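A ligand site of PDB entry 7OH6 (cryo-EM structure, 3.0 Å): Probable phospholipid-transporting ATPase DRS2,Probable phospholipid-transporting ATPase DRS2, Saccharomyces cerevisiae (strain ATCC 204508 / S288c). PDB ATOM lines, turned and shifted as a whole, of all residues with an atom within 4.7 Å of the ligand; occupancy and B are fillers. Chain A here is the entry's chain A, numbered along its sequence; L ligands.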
ATOM      1  N   GLN A 237     -32.796   2.229 -22.077  1.00  0.00           N
ATOM      2  CA  GLN A 237     -32.955   1.457 -23.300  1.00  0.00           C
ATOM      3  C   GLN A 237     -34.348   1.589 -23.911  1.00  0.00           C
ATOM      4  O   GLN A 237     -34.544   1.149 -25.054  1.00  0.00           O
ATOM      5  CB  GLN A 237     -32.650  -0.011 -23.013  1.00  0.00           C
ATOM      6  CG  GLN A 237     -32.319  -0.845 -24.240  1.00  0.00           C
ATOM      7  CD  GLN A 237     -31.936  -2.267 -23.876  1.00  0.00           C
ATOM      8  OE1 GLN A 237     -31.865  -2.627 -22.707  1.00  0.00           O
ATOM      9  NE2 GLN A 237     -31.691  -3.091 -24.891  1.00  0.00           N
ATOM     10  N   THR A 245     -30.560  -3.174 -29.395  1.00  0.00           N
ATOM     11  CA  THR A 245     -31.089  -4.489 -29.048  1.00  0.00           C
ATOM     12  C   THR A 245     -32.530  -4.342 -28.575  1.00  0.00           C
ATOM     13  O   THR A 245     -33.093  -3.238 -28.546  1.00  0.00           O
ATOM     14  CB  THR A 245     -30.218  -5.159 -27.987  1.00  0.00           C
ATOM     15  OG1 THR A 245     -28.902  -4.595 -28.016  1.00  0.00           O
ATOM     16  CG2 THR A 245     -30.112  -6.652 -28.240  1.00  0.00           C
ATOM     17  N   THR A 249     -35.777  -7.426 -22.802  1.00  0.00           N
ATOM     18  CA  THR A 249     -35.030  -8.561 -22.278  1.00  0.00           C
ATOM     19  C   THR A 249     -34.450  -8.271 -20.902  1.00  0.00           C
ATOM     20  O   THR A 249     -34.663  -9.028 -19.948  1.00  0.00           O
ATOM     21  CB  THR A 249     -33.921  -8.952 -23.266  1.00  0.00           C
ATOM     22  OG1 THR A 249     -33.078  -7.815 -23.506  1.00  0.00           O
ATOM     23  CG2 THR A 249     -34.515  -9.435 -24.574  1.00  0.00           C
ATOM     24  N   THR A 250     -33.707  -7.166 -20.782  1.00  0.00           N
ATOM     25  CA  THR A 250     -33.055  -6.846 -19.517  1.00  0.00           C
ATOM     26  C   THR A 250     -34.085  -6.585 -18.418  1.00  0.00           C
ATOM     27  O   THR A 250     -33.991  -7.149 -17.323  1.00  0.00           O
ATOM     28  CB  THR A 250     -32.140  -5.634 -19.684  1.00  0.00           C
ATOM     29  OG1 THR A 250     -32.923  -4.470 -19.934  1.00  0.00           O
ATOM     30  CG2 THR A 250     -31.180  -5.851 -20.849  1.00  0.00           C
ATOM     31  N   THR A 253     -35.889  -9.912 -17.435  1.00  0.00           N
ATOM     32  CA  THR A 253     -35.141 -10.769 -16.521  1.00  0.00           C
ATOM     33  C   THR A 253     -35.017 -10.126 -15.147  1.00  0.00           C
ATOM     34  O   THR A 253     -35.047 -10.823 -14.122  1.00  0.00           O
ATOM     35  CB  THR A 253     -33.755 -11.061 -17.100  1.00  0.00           C
ATOM     36  OG1 THR A 253     -33.061  -9.834 -17.321  1.00  0.00           O
ATOM     37  CG2 THR A 253     -33.879 -11.819 -18.406  1.00  0.00           C
ATOM     38  N   ASN A 504     -22.711  -3.725 -21.674  1.00  0.00           N
ATOM     39  CA  ASN A 504     -22.585  -5.167 -21.522  1.00  0.00           C
ATOM     40  C   ASN A 504     -21.422  -5.574 -20.641  1.00  0.00           C
ATOM     41  O   ASN A 504     -21.227  -6.785 -20.433  1.00  0.00           O
ATOM     42  CB  ASN A 504     -22.453  -5.823 -22.897  1.00  0.00           C
ATOM     43  CG  ASN A 504     -23.691  -5.654 -23.751  1.00  0.00           C
ATOM     44  OD1 ASN A 504     -24.580  -6.512 -23.759  1.00  0.00           O
ATOM     45  ND2 ASN A 504     -23.761  -4.536 -24.469  1.00  0.00           N
ATOM     46  N   PRO A 507     -23.019  -7.660 -17.158  1.00  0.00           N
ATOM     47  CA  PRO A 507     -24.191  -8.371 -17.679  1.00  0.00           C
ATOM     48  C   PRO A 507     -25.073  -8.898 -16.553  1.00  0.00           C
ATOM     49  O   PRO A 507     -24.681  -8.948 -15.392  1.00  0.00           O
ATOM     50  CB  PRO A 507     -23.571  -9.514 -18.484  1.00  0.00           C
ATOM     51  CG  PRO A 507     -22.289  -9.796 -17.772  1.00  0.00           C
ATOM     52  CD  PRO A 507     -21.791  -8.473 -17.246  1.00  0.00           C
ATOM     53  N   ILE A 508     -26.287  -9.287 -16.933  1.00  0.00           N
ATOM     54  CA  ILE A 508     -27.210  -9.904 -16.003  1.00  0.00           C
ATOM     55  C   ILE A 508     -27.204 -11.425 -16.111  1.00  0.00           C
ATOM     56  O   ILE A 508     -27.607 -12.102 -15.142  1.00  0.00           O
ATOM     57  CB  ILE A 508     -28.644  -9.350 -16.213  1.00  0.00           C
ATOM     58  CG1 ILE A 508     -29.529  -9.659 -15.013  1.00  0.00           C
ATOM     59  CG2 ILE A 508     -29.248  -9.899 -17.497  1.00  0.00           C
ATOM     60  CD1 ILE A 508     -30.871  -8.960 -15.052  1.00  0.00           C
ATOM     61  N   SER A 509     -26.747 -11.983 -17.232  1.00  0.00           N
ATOM     62  CA  SER A 509     -26.585 -13.428 -17.328  1.00  0.00           C
ATOM     63  C   SER A 509     -25.609 -13.936 -16.270  1.00  0.00           C
ATOM     64  O   SER A 509     -25.807 -15.020 -15.702  1.00  0.00           O
ATOM     65  CB  SER A 509     -26.110 -13.819 -18.726  1.00  0.00           C
ATOM     66  OG  SER A 509     -24.833 -13.279 -18.997  1.00  0.00           O
ATOM     67  N   VAL A 512     -27.484 -14.072 -12.939  1.00  0.00           N
ATOM     68  CA  VAL A 512     -28.423 -15.172 -12.773  1.00  0.00           C
ATOM     69  C   VAL A 512     -27.706 -16.526 -12.741  1.00  0.00           C
ATOM     70  O   VAL A 512     -28.132 -17.443 -12.020  1.00  0.00           O
ATOM     71  CB  VAL A 512     -29.518 -15.150 -13.856  1.00  0.00           C
ATOM     72  CG1 VAL A 512     -30.262 -13.822 -13.817  1.00  0.00           C
ATOM     73  CG2 VAL A 512     -28.929 -15.396 -15.227  1.00  0.00           C
ATOM     74  N   THR A 513     -26.603 -16.662 -13.476  1.00  0.00           N
ATOM     75  CA  THR A 513     -25.856 -17.912 -13.442  1.00  0.00           C
ATOM     76  C   THR A 513     -25.150 -18.106 -12.112  1.00  0.00           C
ATOM     77  O   THR A 513     -24.979 -19.242 -11.668  1.00  0.00           O
ATOM     78  CB  THR A 513     -24.840 -17.962 -14.581  1.00  0.00           C
ATOM     79  OG1 THR A 513     -24.102 -16.736 -14.626  1.00  0.00           O
ATOM     80  CG2 THR A 513     -25.541 -18.189 -15.913  1.00  0.00           C
ATOM     81  N   LEU A 516     -27.890 -19.575  -9.948  1.00  0.00           N
ATOM     82  CA  LEU A 516     -28.146 -20.953 -10.327  1.00  0.00           C
ATOM     83  C   LEU A 516     -27.017 -21.865  -9.868  1.00  0.00           C
ATOM     84  O   LEU A 516     -27.271 -22.981  -9.379  1.00  0.00           O
ATOM     85  CB  LEU A 516     -28.349 -21.063 -11.834  1.00  0.00           C
ATOM     86  CG  LEU A 516     -29.598 -20.401 -12.411  1.00  0.00           C
ATOM     87  CD1 LEU A 516     -29.724 -20.701 -13.897  1.00  0.00           C
ATOM     88  CD2 LEU A 516     -30.832 -20.835 -11.661  1.00  0.00           C
ATOM     89  N   TYR A1023     -17.475  -7.633 -26.336  1.00  0.00           N
ATOM     90  CA  TYR A1023     -18.072  -6.313 -26.511  1.00  0.00           C
ATOM     91  C   TYR A1023     -17.033  -5.203 -26.579  1.00  0.00           C
ATOM     92  O   TYR A1023     -17.336  -4.116 -27.075  1.00  0.00           O
ATOM     93  CB  TYR A1023     -19.073  -6.041 -25.390  1.00  0.00           C
ATOM     94  CG  TYR A1023     -20.290  -6.923 -25.472  1.00  0.00           C
ATOM     95  CD1 TYR A1023     -21.381  -6.543 -26.241  1.00  0.00           C
ATOM     96  CD2 TYR A1023     -20.347  -8.135 -24.795  1.00  0.00           C
ATOM     97  CE1 TYR A1023     -22.503  -7.354 -26.331  1.00  0.00           C
ATOM     98  CE2 TYR A1023     -21.465  -8.938 -24.881  1.00  0.00           C
ATOM     99  CZ  TYR A1023     -22.537  -8.547 -25.642  1.00  0.00           C
ATOM    100  OH  TYR A1023     -23.646  -9.356 -25.727  1.00  0.00           O
ATOM    101  N   MET A1046     -25.959 -11.023 -30.887  1.00  0.00           N
ATOM    102  CA  MET A1046     -25.400 -10.484 -29.662  1.00  0.00           C
ATOM    103  C   MET A1046     -26.190 -10.919 -28.442  1.00  0.00           C
ATOM    104  O   MET A1046     -25.623 -11.069 -27.349  1.00  0.00           O
ATOM    105  CB  MET A1046     -25.341  -8.961 -29.738  1.00  0.00           C
ATOM    106  CG  MET A1046     -24.286  -8.423 -30.690  1.00  0.00           C
ATOM    107  SD  MET A1046     -24.419  -6.633 -30.900  1.00  0.00           S
ATOM    108  CE  MET A1046     -24.372  -6.091 -29.208  1.00  0.00           C
ATOM    109  N   SER A1047     -27.497 -11.140 -28.596  1.00  0.00           N
ATOM    110  CA  SER A1047     -28.294 -11.649 -27.483  1.00  0.00           C
ATOM    111  C   SER A1047     -28.080 -13.149 -27.285  1.00  0.00           C
ATOM    112  O   SER A1047     -27.982 -13.623 -26.146  1.00  0.00           O
ATOM    113  CB  SER A1047     -29.773 -11.355 -27.715  1.00  0.00           C
ATOM    114  OG  SER A1047     -30.031  -9.959 -27.662  1.00  0.00           O
ATOM    115  N   ASN A1050     -24.894 -14.833 -24.996  1.00  0.00           N
ATOM    116  CA  ASN A1050     -24.961 -15.182 -23.576  1.00  0.00           C
ATOM    117  C   ASN A1050     -26.107 -16.138 -23.258  1.00  0.00           C
ATOM    118  O   ASN A1050     -26.503 -16.237 -22.093  1.00  0.00           O
ATOM    119  CB  ASN A1050     -25.100 -13.917 -22.734  1.00  0.00           C
ATOM    120  CG  ASN A1050     -23.835 -13.086 -22.713  1.00  0.00           C
ATOM    121  OD1 ASN A1050     -22.739 -13.608 -22.900  1.00  0.00           O
ATOM    122  ND2 ASN A1050     -23.983 -11.793 -22.479  1.00  0.00           N
ATOM    123  N   LEU A1051     -26.652 -16.822 -24.245  1.00  0.00           N
ATOM    124  CA  LEU A1051     -27.773 -17.714 -23.967  1.00  0.00           C
ATOM    125  C   LEU A1051     -27.538 -19.148 -24.424  1.00  0.00           C
ATOM    126  O   LEU A1051     -27.925 -20.083 -23.716  1.00  0.00           O
ATOM    127  CB  LEU A1051     -29.064 -17.191 -24.624  1.00  0.00           C
ATOM    128  CG  LEU A1051     -29.980 -16.311 -23.780  1.00  0.00           C
ATOM    129  CD1 LEU A1051     -29.351 -14.958 -23.507  1.00  0.00           C
ATOM    130  CD2 LEU A1051     -31.322 -16.137 -24.472  1.00  0.00           C
ATOM    131  N   PHE A1052     -26.928 -19.348 -25.584  1.00  0.00           N
ATOM    132  CA  PHE A1052     -26.834 -20.680 -26.178  1.00  0.00           C
ATOM    133  C   PHE A1052     -25.420 -21.210 -26.290  1.00  0.00           C
ATOM    134  O   PHE A1052     -25.235 -22.432 -26.303  1.00  0.00           O
ATOM    135  CB  PHE A1052     -27.474 -20.695 -27.569  1.00  0.00           C
ATOM    136  CG  PHE A1052     -28.942 -20.389 -27.581  1.00  0.00           C
ATOM    137  CD1 PHE A1052     -29.714 -20.539 -26.448  1.00  0.00           C
ATOM    138  CD2 PHE A1052     -29.558 -19.940 -28.736  1.00  0.00           C
ATOM    139  CE1 PHE A1052     -31.064 -20.253 -26.461  1.00  0.00           C
ATOM    140  CE2 PHE A1052     -30.904 -19.652 -28.757  1.00  0.00           C
ATOM    141  CZ  PHE A1052     -31.658 -19.807 -27.609  1.00  0.00           C
ATOM    142  N   VAL A1055     -22.960 -20.532 -21.967  1.00  0.00           N
ATOM    143  CA  VAL A1055     -23.674 -20.693 -20.712  1.00  0.00           C
ATOM    144  C   VAL A1055     -23.254 -21.985 -20.036  1.00  0.00           C
ATOM    145  O   VAL A1055     -23.331 -22.114 -18.803  1.00  0.00           O
ATOM    146  CB  VAL A1055     -25.204 -20.660 -20.927  1.00  0.00           C
ATOM    147  CG1 VAL A1055     -25.649 -19.262 -21.295  1.00  0.00           C
ATOM    148  CG2 VAL A1055     -25.597 -21.652 -22.006  1.00  0.00           C
ATOM    149  N   TRP A1056     -22.793 -22.959 -20.817  1.00  0.00           N
ATOM    150  CA  TRP A1056     -22.429 -24.259 -20.279  1.00  0.00           C
ATOM    151  C   TRP A1056     -21.026 -24.285 -19.671  1.00  0.00           C
ATOM    152  O   TRP A1056     -20.820 -24.996 -18.674  1.00  0.00           O
ATOM    153  CB  TRP A1056     -22.560 -25.344 -21.354  1.00  0.00           C
ATOM    154  CG  TRP A1056     -23.938 -25.490 -21.909  1.00  0.00           C
ATOM    155  CD1 TRP A1056     -24.305 -25.416 -23.217  1.00  0.00           C
ATOM    156  CD2 TRP A1056     -25.153 -25.711 -21.165  1.00  0.00           C
ATOM    157  NE1 TRP A1056     -25.652 -25.601 -23.342  1.00  0.00           N
ATOM    158  CE2 TRP A1056     -26.199 -25.783 -22.094  1.00  0.00           C
ATOM    159  CE3 TRP A1056     -25.436 -25.870 -19.809  1.00  0.00           C
ATOM    160  CZ2 TRP A1056     -27.522 -25.997 -21.715  1.00  0.00           C
ATOM    161  CZ3 TRP A1056     -26.755 -26.076 -19.426  1.00  0.00           C
ATOM    162  CH2 TRP A1056     -27.779 -26.138 -20.378  1.00  0.00           C
ATOM    163  N   PHE A1059     -21.185 -23.122 -15.950  1.00  0.00           N
ATOM    164  CA  PHE A1059     -21.772 -24.097 -15.045  1.00  0.00           C
ATOM    165  C   PHE A1059     -20.851 -25.298 -14.838  1.00  0.00           C
ATOM    166  O   PHE A1059     -20.673 -25.763 -13.714  1.00  0.00           O
ATOM    167  CB  PHE A1059     -23.134 -24.547 -15.572  1.00  0.00           C
ATOM    168  CG  PHE A1059     -24.255 -23.619 -15.231  1.00  0.00           C
ATOM    169  CD1 PHE A1059     -24.922 -23.738 -14.025  1.00  0.00           C
ATOM    170  CD2 PHE A1059     -24.628 -22.617 -16.102  1.00  0.00           C
ATOM    171  CE1 PHE A1059     -25.952 -22.879 -13.705  1.00  0.00           C
ATOM    172  CE2 PHE A1059     -25.658 -21.758 -15.781  1.00  0.00           C
ATOM    173  CZ  PHE A1059     -26.318 -21.888 -14.587  1.00  0.00           C
ATOM    174  N   PHE A1171     -22.161 -26.689 -31.562  1.00  0.00           N
ATOM    175  CA  PHE A1171     -23.504 -26.130 -31.561  1.00  0.00           C
ATOM    176  C   PHE A1171     -23.575 -24.879 -32.418  1.00  0.00           C
ATOM    177  O   PHE A1171     -24.472 -24.734 -33.249  1.00  0.00           O
ATOM    178  CB  PHE A1171     -23.930 -25.821 -30.124  1.00  0.00           C
ATOM    179  CG  PHE A1171     -25.348 -25.330 -30.001  1.00  0.00           C
ATOM    180  CD1 PHE A1171     -26.339 -25.800 -30.848  1.00  0.00           C
ATOM    181  CD2 PHE A1171     -25.682 -24.380 -29.047  1.00  0.00           C
ATOM    182  CE1 PHE A1171     -27.631 -25.341 -30.737  1.00  0.00           C
ATOM    183  CE2 PHE A1171     -26.977 -23.923 -28.927  1.00  0.00           C
ATOM    184  CZ  PHE A1171     -27.952 -24.403 -29.772  1.00  0.00           C
HETATM  185  C1  LIG L   1     -30.446 -22.284 -20.964  1.00  0.00           C
HETATM  186  C2  LIG L   1     -30.055 -19.841 -18.032  1.00  0.00           C
HETATM  187  C3  LIG L   1     -28.508 -17.907 -18.420  1.00  0.00           C
HETATM  188  C4  LIG L   1     -29.106 -16.111 -20.049  1.00  0.00           C
HETATM  189  C5  LIG L   1     -30.480 -12.799 -19.435  1.00  0.00           C
HETATM  190  C6  LIG L   1     -30.759 -12.278 -20.844  1.00  0.00           C
HETATM  191  C7  LIG L   1     -30.788 -21.886 -22.401  1.00  0.00           C
HETATM  192  C8  LIG L   1     -29.929 -21.066 -20.211  1.00  0.00           C
HETATM  193  C9  LIG L   1     -30.306 -21.173 -18.731  1.00  0.00           C
HETATM  194  C10 LIG L   1     -28.604 -19.422 -18.226  1.00  0.00           C
HETATM  195  C11 LIG L   1     -29.512 -17.463 -19.491  1.00  0.00           C
HETATM  196  C12 LIG L   1     -29.689 -14.990 -19.184  1.00  0.00           C
HETATM  197  C13 LIG L   1     -29.430 -11.982 -21.545  1.00  0.00           C
HETATM  198  C14 LIG L   1     -28.186  -7.942 -21.486  1.00  0.00           C
HETATM  199  C15 LIG L   1     -28.439  -7.735 -22.974  1.00  0.00           C
HETATM  200  C16 LIG L   1     -28.607  -6.239 -23.255  1.00  0.00           C
HETATM  201  C17 LIG L   1     -32.737 -12.889 -21.953  1.00  0.00           C
HETATM  202  C18 LIG L   1     -33.657 -13.898 -22.641  1.00  0.00           C
HETATM  203  C19 LIG L   1     -33.760 -15.158 -21.785  1.00  0.00           C
HETATM  204  C20 LIG L   1     -34.443 -14.827 -20.455  1.00  0.00           C
HETATM  205  C21 LIG L   1     -34.148 -15.913 -19.424  1.00  0.00           C
HETATM  206  C22 LIG L   1     -34.570 -15.424 -18.040  1.00  0.00           C
HETATM  207  C23 LIG L   1     -33.839 -16.215 -16.965  1.00  0.00           C
HETATM  208  C24 LIG L   1     -34.381 -17.636 -16.906  1.00  0.00           C
HETATM  209  C25 LIG L   1     -34.404 -18.111 -15.449  1.00  0.00           C
HETATM  210  N1  LIG L   1     -29.649  -8.438 -23.376  1.00  0.00           N
HETATM  211  O1  LIG L   1     -30.400 -15.249 -18.284  1.00  0.00           O
HETATM  212  O2  LIG L   1     -29.369 -13.652 -19.471  1.00  0.00           O
HETATM  213  O3  LIG L   1     -28.892 -10.780 -21.079  1.00  0.00           O
HETATM  214  O4  LIG L   1     -26.384 -11.170 -20.607  1.00  0.00           O
HETATM  215  O5  LIG L   1     -27.106 -10.807 -22.931  1.00  0.00           O
HETATM  216  O6  LIG L   1     -27.096  -8.796 -21.315  1.00  0.00           O
HETATM  217  O7  LIG L   1     -29.097  -5.861 -24.355  1.00  0.00           O
HETATM  218  O8  LIG L   1     -28.256  -5.401 -22.397  1.00  0.00           O
HETATM  219  O9  LIG L   1     -31.452 -13.259 -21.562  1.00  0.00           O
HETATM  220  O10 LIG L   1     -33.122 -11.785 -21.762  1.00  0.00           O
HETATM  221  P1  LIG L   1     -27.344 -10.411 -21.492  1.00  0.00           P
HETATM  222  C26 LIG L   1     -30.907 -23.144 -23.257  1.00  0.00           C
HETATM  223  C27 LIG L   1     -29.572 -23.412 -23.942  1.00  0.00           C
HETATM  224  C28 LIG L   1     -29.804 -24.283 -25.179  1.00  0.00           C
HETATM  225  C29 LIG L   1     -29.558 -25.749 -24.814  1.00  0.00           C
HETATM  226  C30 LIG L   1     -29.632 -26.605 -26.074  1.00  0.00           C
HETATM  227  C31 LIG L   1     -28.803 -27.875 -25.869  1.00  0.00           C
HETATM  228  C32 LIG L   1     -29.106 -28.882 -26.978  1.00  0.00           C
HETATM  229  C33 LIG L   1     -34.716 -19.607 -15.412  1.00  0.00           C
HETATM  230  C34 LIG L   1     -35.058 -20.024 -13.976  1.00  0.00           C
HETATM  231  C35 LIG L   1     -35.464 -21.504 -13.964  1.00  0.00           C
HETATM  232  C36 LIG L   1     -35.762 -21.946 -12.530  1.00  0.00           C
HETATM  233  C37 LIG L   1     -34.493 -21.867 -11.692  1.00  0.00           C
HETATM  234  C38 LIG L   1     -34.740 -22.486 -10.318  1.00  0.00           C
HETATM  235  C39 LIG L   1     -28.836 -28.245 -28.341  1.00  0.00           C
HETATM  236  C40 LIG L   1     -34.814 -24.008 -10.461  1.00  0.00           C
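An oxygen (O4) of the ligand sits close to the backbone NH of Ser 509, 3.5 Å away. The side-chain amide nitrogen (ND2) of Asn 1050 is in hydrogen-bond range of an oxygen (O4) of the ligand (3.1 Å). The side-chain hydroxyl (OG1) of Thr 249 sits at hydrogen-bond distance from a nitrogen (N1) of the ligand, at 3.5 Å. OG of Ser 509 sits at hydrogen-bond distance from O4 of the ligand, at 3.1 Å.
OG1 of Thr 250 lies within hydrogen-bond range of OE1 of Gln 237, at 3.5 Å. The backbone carbonyl oxygen (O) of Ser 509 lies within hydrogen-bond range of the side-chain hydroxyl (OG1) of Thr 513, at 2.6 Å. The backbone carbonyl oxygen (O) of Thr 249 sits at hydrogen-bond distance from the side-chain hydroxyl (OG1) of Thr 253, 3.2 Å away. O of Thr 250 lies within hydrogen-bond range of OG1 of Thr 253.
Merely in contact with the ligand: Leu 1051 (3.3 Å), Thr 250 (3.3 Å), Val 512 (3.4 Å), Thr 253 (3.4 Å), Ile 508 (3.7 Å), Trp 1056 (3.7 Å), Leu 516 (3.8 Å), Phe 1052 (3.8 Å), Gln 237 (3.8 Å), Thr 245 (3.9 Å), Pro 507 (3.9 Å), Thr 513 (3.9 Å) and Phe 1171 (3.95 Å). Within 4 Å of the ligand: Gln 237, Thr 245, Thr 249, Thr 250, Thr 253, Pro 507, Ile 508, Ser 509, Val 512, Thr 513, Leu 516, Asn 1050, Leu 1051, Phe 1052, Trp 1056 and Phe 1171.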
